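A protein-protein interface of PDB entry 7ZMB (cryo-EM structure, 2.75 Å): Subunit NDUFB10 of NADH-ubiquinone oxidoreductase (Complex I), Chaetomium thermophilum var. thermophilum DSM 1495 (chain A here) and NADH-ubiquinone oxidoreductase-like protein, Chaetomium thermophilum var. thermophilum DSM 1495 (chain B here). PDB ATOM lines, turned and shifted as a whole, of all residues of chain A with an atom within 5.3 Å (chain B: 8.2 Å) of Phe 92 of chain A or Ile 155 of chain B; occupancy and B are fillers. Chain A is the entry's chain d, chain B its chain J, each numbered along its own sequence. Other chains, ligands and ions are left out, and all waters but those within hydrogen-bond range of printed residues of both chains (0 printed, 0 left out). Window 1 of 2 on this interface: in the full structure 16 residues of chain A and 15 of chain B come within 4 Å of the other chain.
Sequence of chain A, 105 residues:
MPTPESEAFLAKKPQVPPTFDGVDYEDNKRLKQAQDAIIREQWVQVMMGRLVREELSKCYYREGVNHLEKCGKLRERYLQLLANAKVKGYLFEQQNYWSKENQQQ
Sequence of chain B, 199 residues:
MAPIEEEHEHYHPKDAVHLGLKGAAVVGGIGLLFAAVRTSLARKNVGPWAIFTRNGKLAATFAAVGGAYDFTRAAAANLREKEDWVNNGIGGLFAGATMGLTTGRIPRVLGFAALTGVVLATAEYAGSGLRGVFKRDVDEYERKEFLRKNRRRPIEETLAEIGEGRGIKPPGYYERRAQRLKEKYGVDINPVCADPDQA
Of chain B, only Ile 155 (3.3 Å), Thr 158 (3.7 Å), Ile 162 (3.8 Å) and Ile 168 (3.5 Å) come within 4 Å of Phe 92 of chain A. Of chain A, only Phe 92, Asn 96, Tyr 97 and Trp 98 come within 4 Å of Ile 155 of chain B. Of the printed residues of chain A, Pro 154 of chain B touches Tyr 97. Printed residues of chain B within 4 Å of Tyr 97 of chain A: Arg 152, Arg 153, Pro 154 and Ile 155. Printed residues of chain B within 4 Å of Gln 94 of chain A: Arg 151 and Arg 152. Printed residues of chain A within 4 Å of Arg 152 of chain B: Glu 93 (2.4 Å), Gln 94 (3.4 Å), Gln 95 (3.8 Å), Asn 96 (3.0 Å) and Tyr 97 (3.96 Å). Printed residues of chain A within 4 Å of Pro 171 of chain B: Trp 98. Pro 170 of chain B touches none of the printed residues of chain A. The nearest residue of chain B that does not touch Phe 92 of chain A is Leu 159 of chain B (4.4 Å).
The backbone carbonyl oxygen (O) of Phe 92 of chain A lies within hydrogen-bond range of the side-chain amide nitrogen (ND2) of Asn 96 of chain A, 2.9 Å away.
CD1 of Ile 155 of chain B touches CE1 of Phe 92 of chain A (3.3 Å). Ile 162 of chain B touches Phe 92 of chain A. Ile 168 of chain B touches Phe 92 of chain A. Gln 94 of chain A touches Arg 151 of chain B. CA of Arg 152 of chain B touches O of Gln 95 of chain A (3.8 Å). CA of Asn 96 of chain A touches O of Arg 153 of chain B, 3.2 Å away. Asn 96 of chain A touches Ile 155 of chain B. CG2 of Thr 158 of chain B touches OD1 of Asn 96 of chain A, 3.1 Å away. CB of Tyr 97 of chain A touches CZ of Arg 152 of chain B, 3.96 Å away. Trp 98 of chain A touches Pro 171 of chain B.
Of the 9 printed residues of chain A, 7 touch a printed residue of chain B. Hydrophobic or aromatic side chains of chain A that line the printed part of chain B: Phe 92, Tyr 97 and Trp 98. Among the printed residues, 20 pairs touch across the chains.
The backbone carbonyl oxygen (O) of Arg 153 of chain B lies within hydrogen-bond range of the backbone NH (N) of Tyr 97 of chain A (3.1 Å). O of Gln 94 of chain A lies within hydrogen-bond range of NE of Arg 152 of chain B, 3.4 Å away. The backbone carbonyl oxygen of Tyr 97 of chain A is in hydrogen-bond range of the backbone NH of Ile 155 of chain B, 3.0 Å away. NH2 of Arg 152 of chain B is in hydrogen-bond range of O of Asn 96 of chain A. N of Arg 153 of chain B lies within hydrogen-bond range of O of Gln 95 of chain A, at 3.0 Å. The backbone carbonyl oxygen (O) of Glu 93 of chain A lies within hydrogen-bond range of the guanidinium group (NH2) of Arg 152 of chain B, at 2.4 Å.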
ATOM      1  N   TYR A  90      -3.826   8.383  13.252  1.00  0.00           N
ATOM      2  CA  TYR A  90      -3.898   7.658  14.548  1.00  0.00           C
ATOM      3  C   TYR A  90      -3.719   6.157  14.344  1.00  0.00           C
ATOM      4  O   TYR A  90      -3.820   5.430  15.329  1.00  0.00           O
ATOM      5  CB  TYR A  90      -5.292   7.847  15.146  1.00  0.00           C
ATOM      6  CG  TYR A  90      -6.453   7.402  14.290  1.00  0.00           C
ATOM      7  CD1 TYR A  90      -6.783   6.064  14.159  1.00  0.00           C
ATOM      8  CD2 TYR A  90      -7.256   8.325  13.643  1.00  0.00           C
ATOM      9  CE1 TYR A  90      -7.847   5.647  13.379  1.00  0.00           C
ATOM     10  CE2 TYR A  90      -8.333   7.927  12.867  1.00  0.00           C
ATOM     11  CZ  TYR A  90      -8.631   6.583  12.738  1.00  0.00           C
ATOM     12  OH  TYR A  90      -9.686   6.170  11.980  1.00  0.00           O
ATOM     13  N   LEU A  91      -3.457   5.714  13.122  1.00  0.00           N
ATOM     14  CA  LEU A  91      -3.445   4.266  12.811  1.00  0.00           C
ATOM     15  C   LEU A  91      -2.129   3.608  13.227  1.00  0.00           C
ATOM     16  O   LEU A  91      -2.186   2.486  13.736  1.00  0.00           O
ATOM     17  CB  LEU A  91      -3.737   4.110  11.314  1.00  0.00           C
ATOM     18  CG  LEU A  91      -3.939   2.680  10.816  1.00  0.00           C
ATOM     19  CD1 LEU A  91      -5.084   2.007  11.559  1.00  0.00           C
ATOM     20  CD2 LEU A  91      -4.199   2.672   9.320  1.00  0.00           C
ATOM     21  N   PHE A  92      -0.991   4.269  13.033  1.00  0.00           N
ATOM     22  CA  PHE A  92       0.238   3.649  13.509  1.00  0.00           C
ATOM     23  C   PHE A  92       0.264   3.579  15.028  1.00  0.00           C
ATOM     24  O   PHE A  92       0.760   2.604  15.600  1.00  0.00           O
ATOM     25  CB  PHE A  92       1.455   4.400  12.979  1.00  0.00           C
ATOM     26  CG  PHE A  92       2.686   3.564  12.933  1.00  0.00           C
ATOM     27  CD1 PHE A  92       3.512   3.468  14.033  1.00  0.00           C
ATOM     28  CD2 PHE A  92       3.008   2.851  11.799  1.00  0.00           C
ATOM     29  CE1 PHE A  92       4.634   2.692  13.998  1.00  0.00           C
ATOM     30  CE2 PHE A  92       4.129   2.063  11.763  1.00  0.00           C
ATOM     31  CZ  PHE A  92       4.944   1.984  12.866  1.00  0.00           C
ATOM     32  N   GLU A  93      -0.251   4.614  15.697  1.00  0.00           N
ATOM     33  CA  GLU A  93      -0.415   4.569  17.147  1.00  0.00           C
ATOM     34  C   GLU A  93      -1.346   3.438  17.561  1.00  0.00           C
ATOM     35  O   GLU A  93      -1.045   2.685  18.492  1.00  0.00           O
ATOM     36  CB  GLU A  93      -0.974   5.899  17.650  1.00  0.00           C
ATOM     37  CG  GLU A  93      -0.020   7.078  17.627  1.00  0.00           C
ATOM     38  CD  GLU A  93       0.926   7.085  18.801  1.00  0.00           C
ATOM     39  OE1 GLU A  93       0.506   6.677  19.898  1.00  0.00           O
ATOM     40  OE2 GLU A  93       2.080   7.513  18.634  1.00  0.00           O
ATOM     41  N   GLN A  94      -2.476   3.301  16.872  1.00  0.00           N
ATOM     42  CA  GLN A  94      -3.483   2.334  17.279  1.00  0.00           C
ATOM     43  C   GLN A  94      -2.995   0.902  17.138  1.00  0.00           C
ATOM     44  O   GLN A  94      -3.404   0.029  17.910  1.00  0.00           O
ATOM     45  CB  GLN A  94      -4.750   2.541  16.457  1.00  0.00           C
ATOM     46  CG  GLN A  94      -6.008   2.095  17.152  1.00  0.00           C
ATOM     47  CD  GLN A  94      -7.219   2.216  16.276  1.00  0.00           C
ATOM     48  OE1 GLN A  94      -7.630   3.314  15.918  1.00  0.00           O
ATOM     49  NE2 GLN A  94      -7.802   1.085  15.918  1.00  0.00           N
ATOM     50  N   GLN A  95      -2.124   0.638  16.170  1.00  0.00           N
ATOM     51  CA  GLN A  95      -1.733  -0.720  15.841  1.00  0.00           C
ATOM     52  C   GLN A  95      -0.383  -1.125  16.415  1.00  0.00           C
ATOM     53  O   GLN A  95      -0.080  -2.319  16.450  1.00  0.00           O
ATOM     54  CB  GLN A  95      -1.733  -0.895  14.324  1.00  0.00           C
ATOM     55  CG  GLN A  95      -3.072  -0.572  13.708  1.00  0.00           C
ATOM     56  CD  GLN A  95      -3.353  -1.354  12.455  1.00  0.00           C
ATOM     57  OE1 GLN A  95      -4.381  -2.021  12.340  1.00  0.00           O
ATOM     58  NE2 GLN A  95      -2.436  -1.283  11.501  1.00  0.00           N
ATOM     59  N   ASN A  96       0.424  -0.177  16.876  1.00  0.00           N
ATOM     60  CA  ASN A  96       1.729  -0.486  17.441  1.00  0.00           C
ATOM     61  C   ASN A  96       1.882   0.205  18.784  1.00  0.00           C
ATOM     62  O   ASN A  96       1.447   1.343  18.966  1.00  0.00           O
ATOM     63  CB  ASN A  96       2.867  -0.067  16.505  1.00  0.00           C
ATOM     64  CG  ASN A  96       2.614  -0.468  15.077  1.00  0.00           C
ATOM     65  OD1 ASN A  96       2.673  -1.643  14.733  1.00  0.00           O
ATOM     66  ND2 ASN A  96       2.302   0.504  14.239  1.00  0.00           N
ATOM     67  N   TYR A  97       2.487  -0.503  19.731  1.00  0.00           N
ATOM     68  CA  TYR A  97       2.805   0.060  21.037  1.00  0.00           C
ATOM     69  C   TYR A  97       4.319   0.051  21.199  1.00  0.00           C
ATOM     70  O   TYR A  97       4.981  -0.936  20.867  1.00  0.00           O
ATOM     71  CB  TYR A  97       2.104  -0.695  22.168  1.00  0.00           C
ATOM     72  CG  TYR A  97       2.504  -2.143  22.339  1.00  0.00           C
ATOM     73  CD1 TYR A  97       1.831  -3.154  21.668  1.00  0.00           C
ATOM     74  CD2 TYR A  97       3.550  -2.498  23.178  1.00  0.00           C
ATOM     75  CE1 TYR A  97       2.186  -4.477  21.831  1.00  0.00           C
ATOM     76  CE2 TYR A  97       3.919  -3.818  23.339  1.00  0.00           C
ATOM     77  CZ  TYR A  97       3.235  -4.803  22.663  1.00  0.00           C
ATOM     78  OH  TYR A  97       3.597  -6.120  22.823  1.00  0.00           O
ATOM     79  N   TRP A  98       4.860   1.164  21.692  1.00  0.00           N
ATOM     80  CA  TRP A  98       6.307   1.314  21.774  1.00  0.00           C
ATOM     81  C   TRP A  98       6.802   1.117  23.202  1.00  0.00           C
ATOM     82  O   TRP A  98       7.862   0.518  23.420  1.00  0.00           O
ATOM     83  CB  TRP A  98       6.701   2.681  21.222  1.00  0.00           C
ATOM     84  CG  TRP A  98       8.016   3.187  21.680  1.00  0.00           C
ATOM     85  CD1 TRP A  98       9.236   2.620  21.465  1.00  0.00           C
ATOM     86  CD2 TRP A  98       8.254   4.387  22.417  1.00  0.00           C
ATOM     87  NE1 TRP A  98      10.221   3.390  22.034  1.00  0.00           N
ATOM     88  CE2 TRP A  98       9.642   4.481  22.624  1.00  0.00           C
ATOM     89  CE3 TRP A  98       7.426   5.387  22.925  1.00  0.00           C
ATOM     90  CZ2 TRP A  98      10.221   5.539  23.318  1.00  0.00           C
ATOM     91  CZ3 TRP A  98       8.001   6.434  23.614  1.00  0.00           C
ATOM     92  CH2 TRP A  98       9.385   6.502  23.807  1.00  0.00           C
ATOM     93  N   ARG B 151      -5.214  -6.658  18.483  1.00  0.00           N
ATOM     94  CA  ARG B 151      -5.346  -5.370  17.811  1.00  0.00           C
ATOM     95  C   ARG B 151      -4.120  -4.477  17.960  1.00  0.00           C
ATOM     96  O   ARG B 151      -3.845  -3.672  17.065  1.00  0.00           O
ATOM     97  CB  ARG B 151      -6.584  -4.634  18.328  1.00  0.00           C
ATOM     98  CG  ARG B 151      -7.879  -5.308  17.934  1.00  0.00           C
ATOM     99  CD  ARG B 151      -9.088  -4.562  18.454  1.00  0.00           C
ATOM    100  NE  ARG B 151     -10.320  -5.217  18.046  1.00  0.00           N
ATOM    101  CZ  ARG B 151     -10.929  -6.150  18.769  1.00  0.00           C
ATOM    102  NH1 ARG B 151     -12.046  -6.713  18.332  1.00  0.00           N
ATOM    103  NH2 ARG B 151     -10.420  -6.520  19.934  1.00  0.00           N
ATOM    104  N   ARG B 152      -3.385  -4.589  19.060  1.00  0.00           N
ATOM    105  CA  ARG B 152      -2.115  -3.894  19.220  1.00  0.00           C
ATOM    106  C   ARG B 152      -0.978  -4.900  19.144  1.00  0.00           C
ATOM    107  O   ARG B 152      -1.053  -5.983  19.729  1.00  0.00           O
ATOM    108  CB  ARG B 152      -2.043  -3.151  20.552  1.00  0.00           C
ATOM    109  CG  ARG B 152      -3.020  -2.021  20.718  1.00  0.00           C
ATOM    110  CD  ARG B 152      -2.469  -0.967  21.658  1.00  0.00           C
ATOM    111  NE  ARG B 152      -1.858   0.148  20.952  1.00  0.00           N
ATOM    112  CZ  ARG B 152      -1.313   1.204  21.549  1.00  0.00           C
ATOM    113  NH1 ARG B 152      -1.302   1.293  22.867  1.00  0.00           N
ATOM    114  NH2 ARG B 152      -0.777   2.172  20.823  1.00  0.00           N
ATOM    115  N   ARG B 153       0.071  -4.537  18.420  1.00  0.00           N
ATOM    116  CA  ARG B 153       1.239  -5.371  18.219  1.00  0.00           C
ATOM    117  C   ARG B 153       2.485  -4.593  18.604  1.00  0.00           C
ATOM    118  O   ARG B 153       2.507  -3.364  18.506  1.00  0.00           O
ATOM    119  CB  ARG B 153       1.346  -5.832  16.758  1.00  0.00           C
ATOM    120  CG  ARG B 153       0.247  -6.792  16.333  1.00  0.00           C
ATOM    121  CD  ARG B 153       0.395  -7.217  14.880  1.00  0.00           C
ATOM    122  NE  ARG B 153      -0.675  -8.122  14.470  1.00  0.00           N
ATOM    123  CZ  ARG B 153      -0.821  -8.602  13.238  1.00  0.00           C
ATOM    124  NH1 ARG B 153       0.036  -8.261  12.286  1.00  0.00           N
ATOM    125  NH2 ARG B 153      -1.824  -9.421  12.958  1.00  0.00           N
ATOM    126  N   PRO B 154       3.529  -5.280  19.066  1.00  0.00           N
ATOM    127  CA  PRO B 154       4.744  -4.572  19.479  1.00  0.00           C
ATOM    128  C   PRO B 154       5.377  -3.841  18.310  1.00  0.00           C
ATOM    129  O   PRO B 154       5.343  -4.302  17.168  1.00  0.00           O
ATOM    130  CB  PRO B 154       5.644  -5.693  20.006  1.00  0.00           C
ATOM    131  CG  PRO B 154       5.132  -6.921  19.362  1.00  0.00           C
ATOM    132  CD  PRO B 154       3.658  -6.735  19.245  1.00  0.00           C
ATOM    133  N   ILE B 155       5.969  -2.684  18.612  1.00  0.00           N
ATOM    134  CA  ILE B 155       6.514  -1.829  17.566  1.00  0.00           C
ATOM    135  C   ILE B 155       7.602  -2.550  16.787  1.00  0.00           C
ATOM    136  O   ILE B 155       7.812  -2.275  15.602  1.00  0.00           O
ATOM    137  CB  ILE B 155       7.020  -0.511  18.179  1.00  0.00           C
ATOM    138  CG1 ILE B 155       7.504   0.441  17.089  1.00  0.00           C
ATOM    139  CG2 ILE B 155       8.121  -0.777  19.196  1.00  0.00           C
ATOM    140  CD1 ILE B 155       6.410   0.974  16.231  1.00  0.00           C
ATOM    141  N   GLU B 156       8.298  -3.494  17.422  1.00  0.00           N
ATOM    142  CA  GLU B 156       9.341  -4.229  16.718  1.00  0.00           C
ATOM    143  C   GLU B 156       8.768  -5.010  15.545  1.00  0.00           C
ATOM    144  O   GLU B 156       9.386  -5.087  14.477  1.00  0.00           O
ATOM    145  CB  GLU B 156      10.061  -5.167  17.687  1.00  0.00           C
ATOM    146  N   GLU B 157       7.583  -5.593  15.724  1.00  0.00           N
ATOM    147  CA  GLU B 157       7.015  -6.456  14.697  1.00  0.00           C
ATOM    148  C   GLU B 157       6.727  -5.686  13.415  1.00  0.00           C
ATOM    149  O   GLU B 157       7.013  -6.174  12.316  1.00  0.00           O
ATOM    150  CB  GLU B 157       5.749  -7.128  15.225  1.00  0.00           C
ATOM    151  CG  GLU B 157       5.123  -8.115  14.258  1.00  0.00           C
ATOM    152  CD  GLU B 157       3.904  -8.797  14.842  1.00  0.00           C
ATOM    153  OE1 GLU B 157       3.540  -8.480  15.993  1.00  0.00           O
ATOM    154  OE2 GLU B 157       3.308  -9.649  14.150  1.00  0.00           O
ATOM    155  N   THR B 158       6.157  -4.484  13.527  1.00  0.00           N
ATOM    156  CA  THR B 158       5.927  -3.689  12.326  1.00  0.00           C
ATOM    157  C   THR B 158       7.238  -3.206  11.723  1.00  0.00           C
ATOM    158  O   THR B 158       7.396  -3.204  10.497  1.00  0.00           O
ATOM    159  CB  THR B 158       4.994  -2.509  12.619  1.00  0.00           C
ATOM    160  OG1 THR B 158       4.748  -1.780  11.408  1.00  0.00           O
ATOM    161  CG2 THR B 158       5.581  -1.568  13.646  1.00  0.00           C
ATOM    162  N   LEU B 159       8.197  -2.810  12.558  1.00  0.00           N
ATOM    163  CA  LEU B 159       9.455  -2.305  12.024  1.00  0.00           C
ATOM    164  C   LEU B 159      10.188  -3.384  11.243  1.00  0.00           C
ATOM    165  O   LEU B 159      10.784  -3.103  10.199  1.00  0.00           O
ATOM    166  CB  LEU B 159      10.333  -1.756  13.147  1.00  0.00           C
ATOM    167  CG  LEU B 159       9.797  -0.559  13.933  1.00  0.00           C
ATOM    168  CD1 LEU B 159      10.938   0.191  14.599  1.00  0.00           C
ATOM    169  CD2 LEU B 159       8.998   0.372  13.043  1.00  0.00           C
ATOM    170  N   ALA B 160      10.150  -4.624  11.727  1.00  0.00           N
ATOM    171  CA  ALA B 160      10.723  -5.719  10.963  1.00  0.00           C
ATOM    172  C   ALA B 160      10.009  -5.910   9.640  1.00  0.00           C
ATOM    173  O   ALA B 160      10.613  -6.399   8.682  1.00  0.00           O
ATOM    174  CB  ALA B 160      10.674  -7.011  11.777  1.00  0.00           C
ATOM    175  N   GLU B 161       8.741  -5.526   9.568  1.00  0.00           N
ATOM    176  CA  GLU B 161       7.924  -5.744   8.383  1.00  0.00           C
ATOM    177  C   GLU B 161       8.114  -4.617   7.370  1.00  0.00           C
ATOM    178  O   GLU B 161       8.582  -4.848   6.254  1.00  0.00           O
ATOM    179  CB  GLU B 161       6.462  -5.868   8.812  1.00  0.00           C
ATOM    180  CG  GLU B 161       6.004  -7.299   8.982  1.00  0.00           C
ATOM    181  CD  GLU B 161       4.824  -7.413   9.931  1.00  0.00           C
ATOM    182  OE1 GLU B 161       4.357  -6.367  10.428  1.00  0.00           O
ATOM    183  OE2 GLU B 161       4.390  -8.550  10.210  1.00  0.00           O
ATOM    184  N   ILE B 162       7.779  -3.386   7.756  1.00  0.00           N
ATOM    185  CA  ILE B 162       7.798  -2.269   6.824  1.00  0.00           C
ATOM    186  C   ILE B 162       9.092  -1.485   6.880  1.00  0.00           C
ATOM    187  O   ILE B 162       9.302  -0.596   6.047  1.00  0.00           O
ATOM    188  CB  ILE B 162       6.601  -1.330   7.051  1.00  0.00           C
ATOM    189  CG1 ILE B 162       6.579  -0.821   8.487  1.00  0.00           C
ATOM    190  CG2 ILE B 162       5.332  -2.037   6.716  1.00  0.00           C
ATOM    191  CD1 ILE B 162       5.526   0.212   8.731  1.00  0.00           C
ATOM    192  N   GLY B 163       9.968  -1.789   7.824  1.00  0.00           N
ATOM    193  CA  GLY B 163      11.223  -1.087   7.915  1.00  0.00           C
ATOM    194  C   GLY B 163      11.121   0.133   8.794  1.00  0.00           C
ATOM    195  O   GLY B 163      10.531   0.087   9.874  1.00  0.00           O
ATOM    196  N   GLU B 164      11.697   1.236   8.339  1.00  0.00           N
ATOM    197  CA  GLU B 164      11.714   2.457   9.121  1.00  0.00           C
ATOM    198  C   GLU B 164      11.944   3.607   8.157  1.00  0.00           C
ATOM    199  O   GLU B 164      12.718   3.478   7.206  1.00  0.00           O
ATOM    200  CB  GLU B 164      12.800   2.388  10.197  1.00  0.00           C
ATOM    201  CG  GLU B 164      12.662   3.381  11.320  1.00  0.00           C
ATOM    202  CD  GLU B 164      13.878   3.383  12.225  1.00  0.00           C
ATOM    203  OE1 GLU B 164      13.993   4.283  13.082  1.00  0.00           O
ATOM    204  OE2 GLU B 164      14.725   2.477  12.080  1.00  0.00           O
ATOM    205  N   GLY B 165      11.266   4.712   8.392  1.00  0.00           N
ATOM    206  CA  GLY B 165      11.228   5.767   7.412  1.00  0.00           C
ATOM    207  C   GLY B 165      10.039   5.631   6.488  1.00  0.00           C
ATOM    208  O   GLY B 165       9.138   4.813   6.687  1.00  0.00           O
ATOM    209  N   GLY B 167       7.825   7.857   6.344  1.00  0.00           N
ATOM    210  CA  GLY B 167       6.776   8.202   7.267  1.00  0.00           C
ATOM    211  C   GLY B 167       6.775   7.396   8.543  1.00  0.00           C
ATOM    212  O   GLY B 167       6.118   7.792   9.508  1.00  0.00           O
ATOM    213  N   ILE B 168       7.483   6.273   8.571  1.00  0.00           N
ATOM    214  CA  ILE B 168       7.637   5.487   9.803  1.00  0.00           C
ATOM    215  C   ILE B 168       8.889   6.022  10.481  1.00  0.00           C
ATOM    216  O   ILE B 168       9.998   5.507  10.336  1.00  0.00           O
ATOM    217  CB  ILE B 168       7.705   3.984   9.527  1.00  0.00           C
ATOM    218  CG1 ILE B 168       6.623   3.587   8.523  1.00  0.00           C
ATOM    219  CG2 ILE B 168       7.555   3.205  10.811  1.00  0.00           C
ATOM    220  CD1 ILE B 168       5.224   3.928   8.958  1.00  0.00           C
ATOM    221  N   LYS B 169       8.708   7.100  11.236  1.00  0.00           N
ATOM    222  CA  LYS B 169       9.807   7.758  11.934  1.00  0.00           C
ATOM    223  C   LYS B 169       9.537   7.620  13.421  1.00  0.00           C
ATOM    224  O   LYS B 169       8.888   8.482  14.027  1.00  0.00           O
ATOM    225  CB  LYS B 169       9.924   9.224  11.518  1.00  0.00           C
ATOM    226  CG  LYS B 169      10.124   9.394  10.024  1.00  0.00           C
ATOM    227  CD  LYS B 169      11.170  10.451   9.704  1.00  0.00           C
ATOM    228  CE  LYS B 169      10.767  11.826  10.210  1.00  0.00           C
ATOM    229  NZ  LYS B 169       9.584  12.360   9.481  1.00  0.00           N
ATOM    230  N   PRO B 170       9.988   6.538  14.046  1.00  0.00           N
ATOM    231  CA  PRO B 170       9.623   6.258  15.425  1.00  0.00           C
ATOM    232  C   PRO B 170      10.443   7.116  16.368  1.00  0.00           C
ATOM    233  O   PRO B 170      11.428   7.731  15.938  1.00  0.00           O
ATOM    234  CB  PRO B 170       9.970   4.767  15.575  1.00  0.00           C
ATOM    235  CG  PRO B 170      10.161   4.264  14.183  1.00  0.00           C
ATOM    236  CD  PRO B 170      10.718   5.415  13.447  1.00  0.00           C
ATOM    237  N   PRO B 171      10.095   7.178  17.652  1.00  0.00           N
ATOM    238  CA  PRO B 171      10.969   7.890  18.583  1.00  0.00           C
ATOM    239  C   PRO B 171      12.343   7.241  18.623  1.00  0.00           C
ATOM    240  O   PRO B 171      12.482   6.039  18.856  1.00  0.00           O
ATOM    241  CB  PRO B 171      10.223   7.782  19.912  1.00  0.00           C
ATOM    242  CG  PRO B 171       9.551   6.480  19.833  1.00  0.00           C
ATOM    243  CD  PRO B 171       9.151   6.308  18.377  1.00  0.00           C
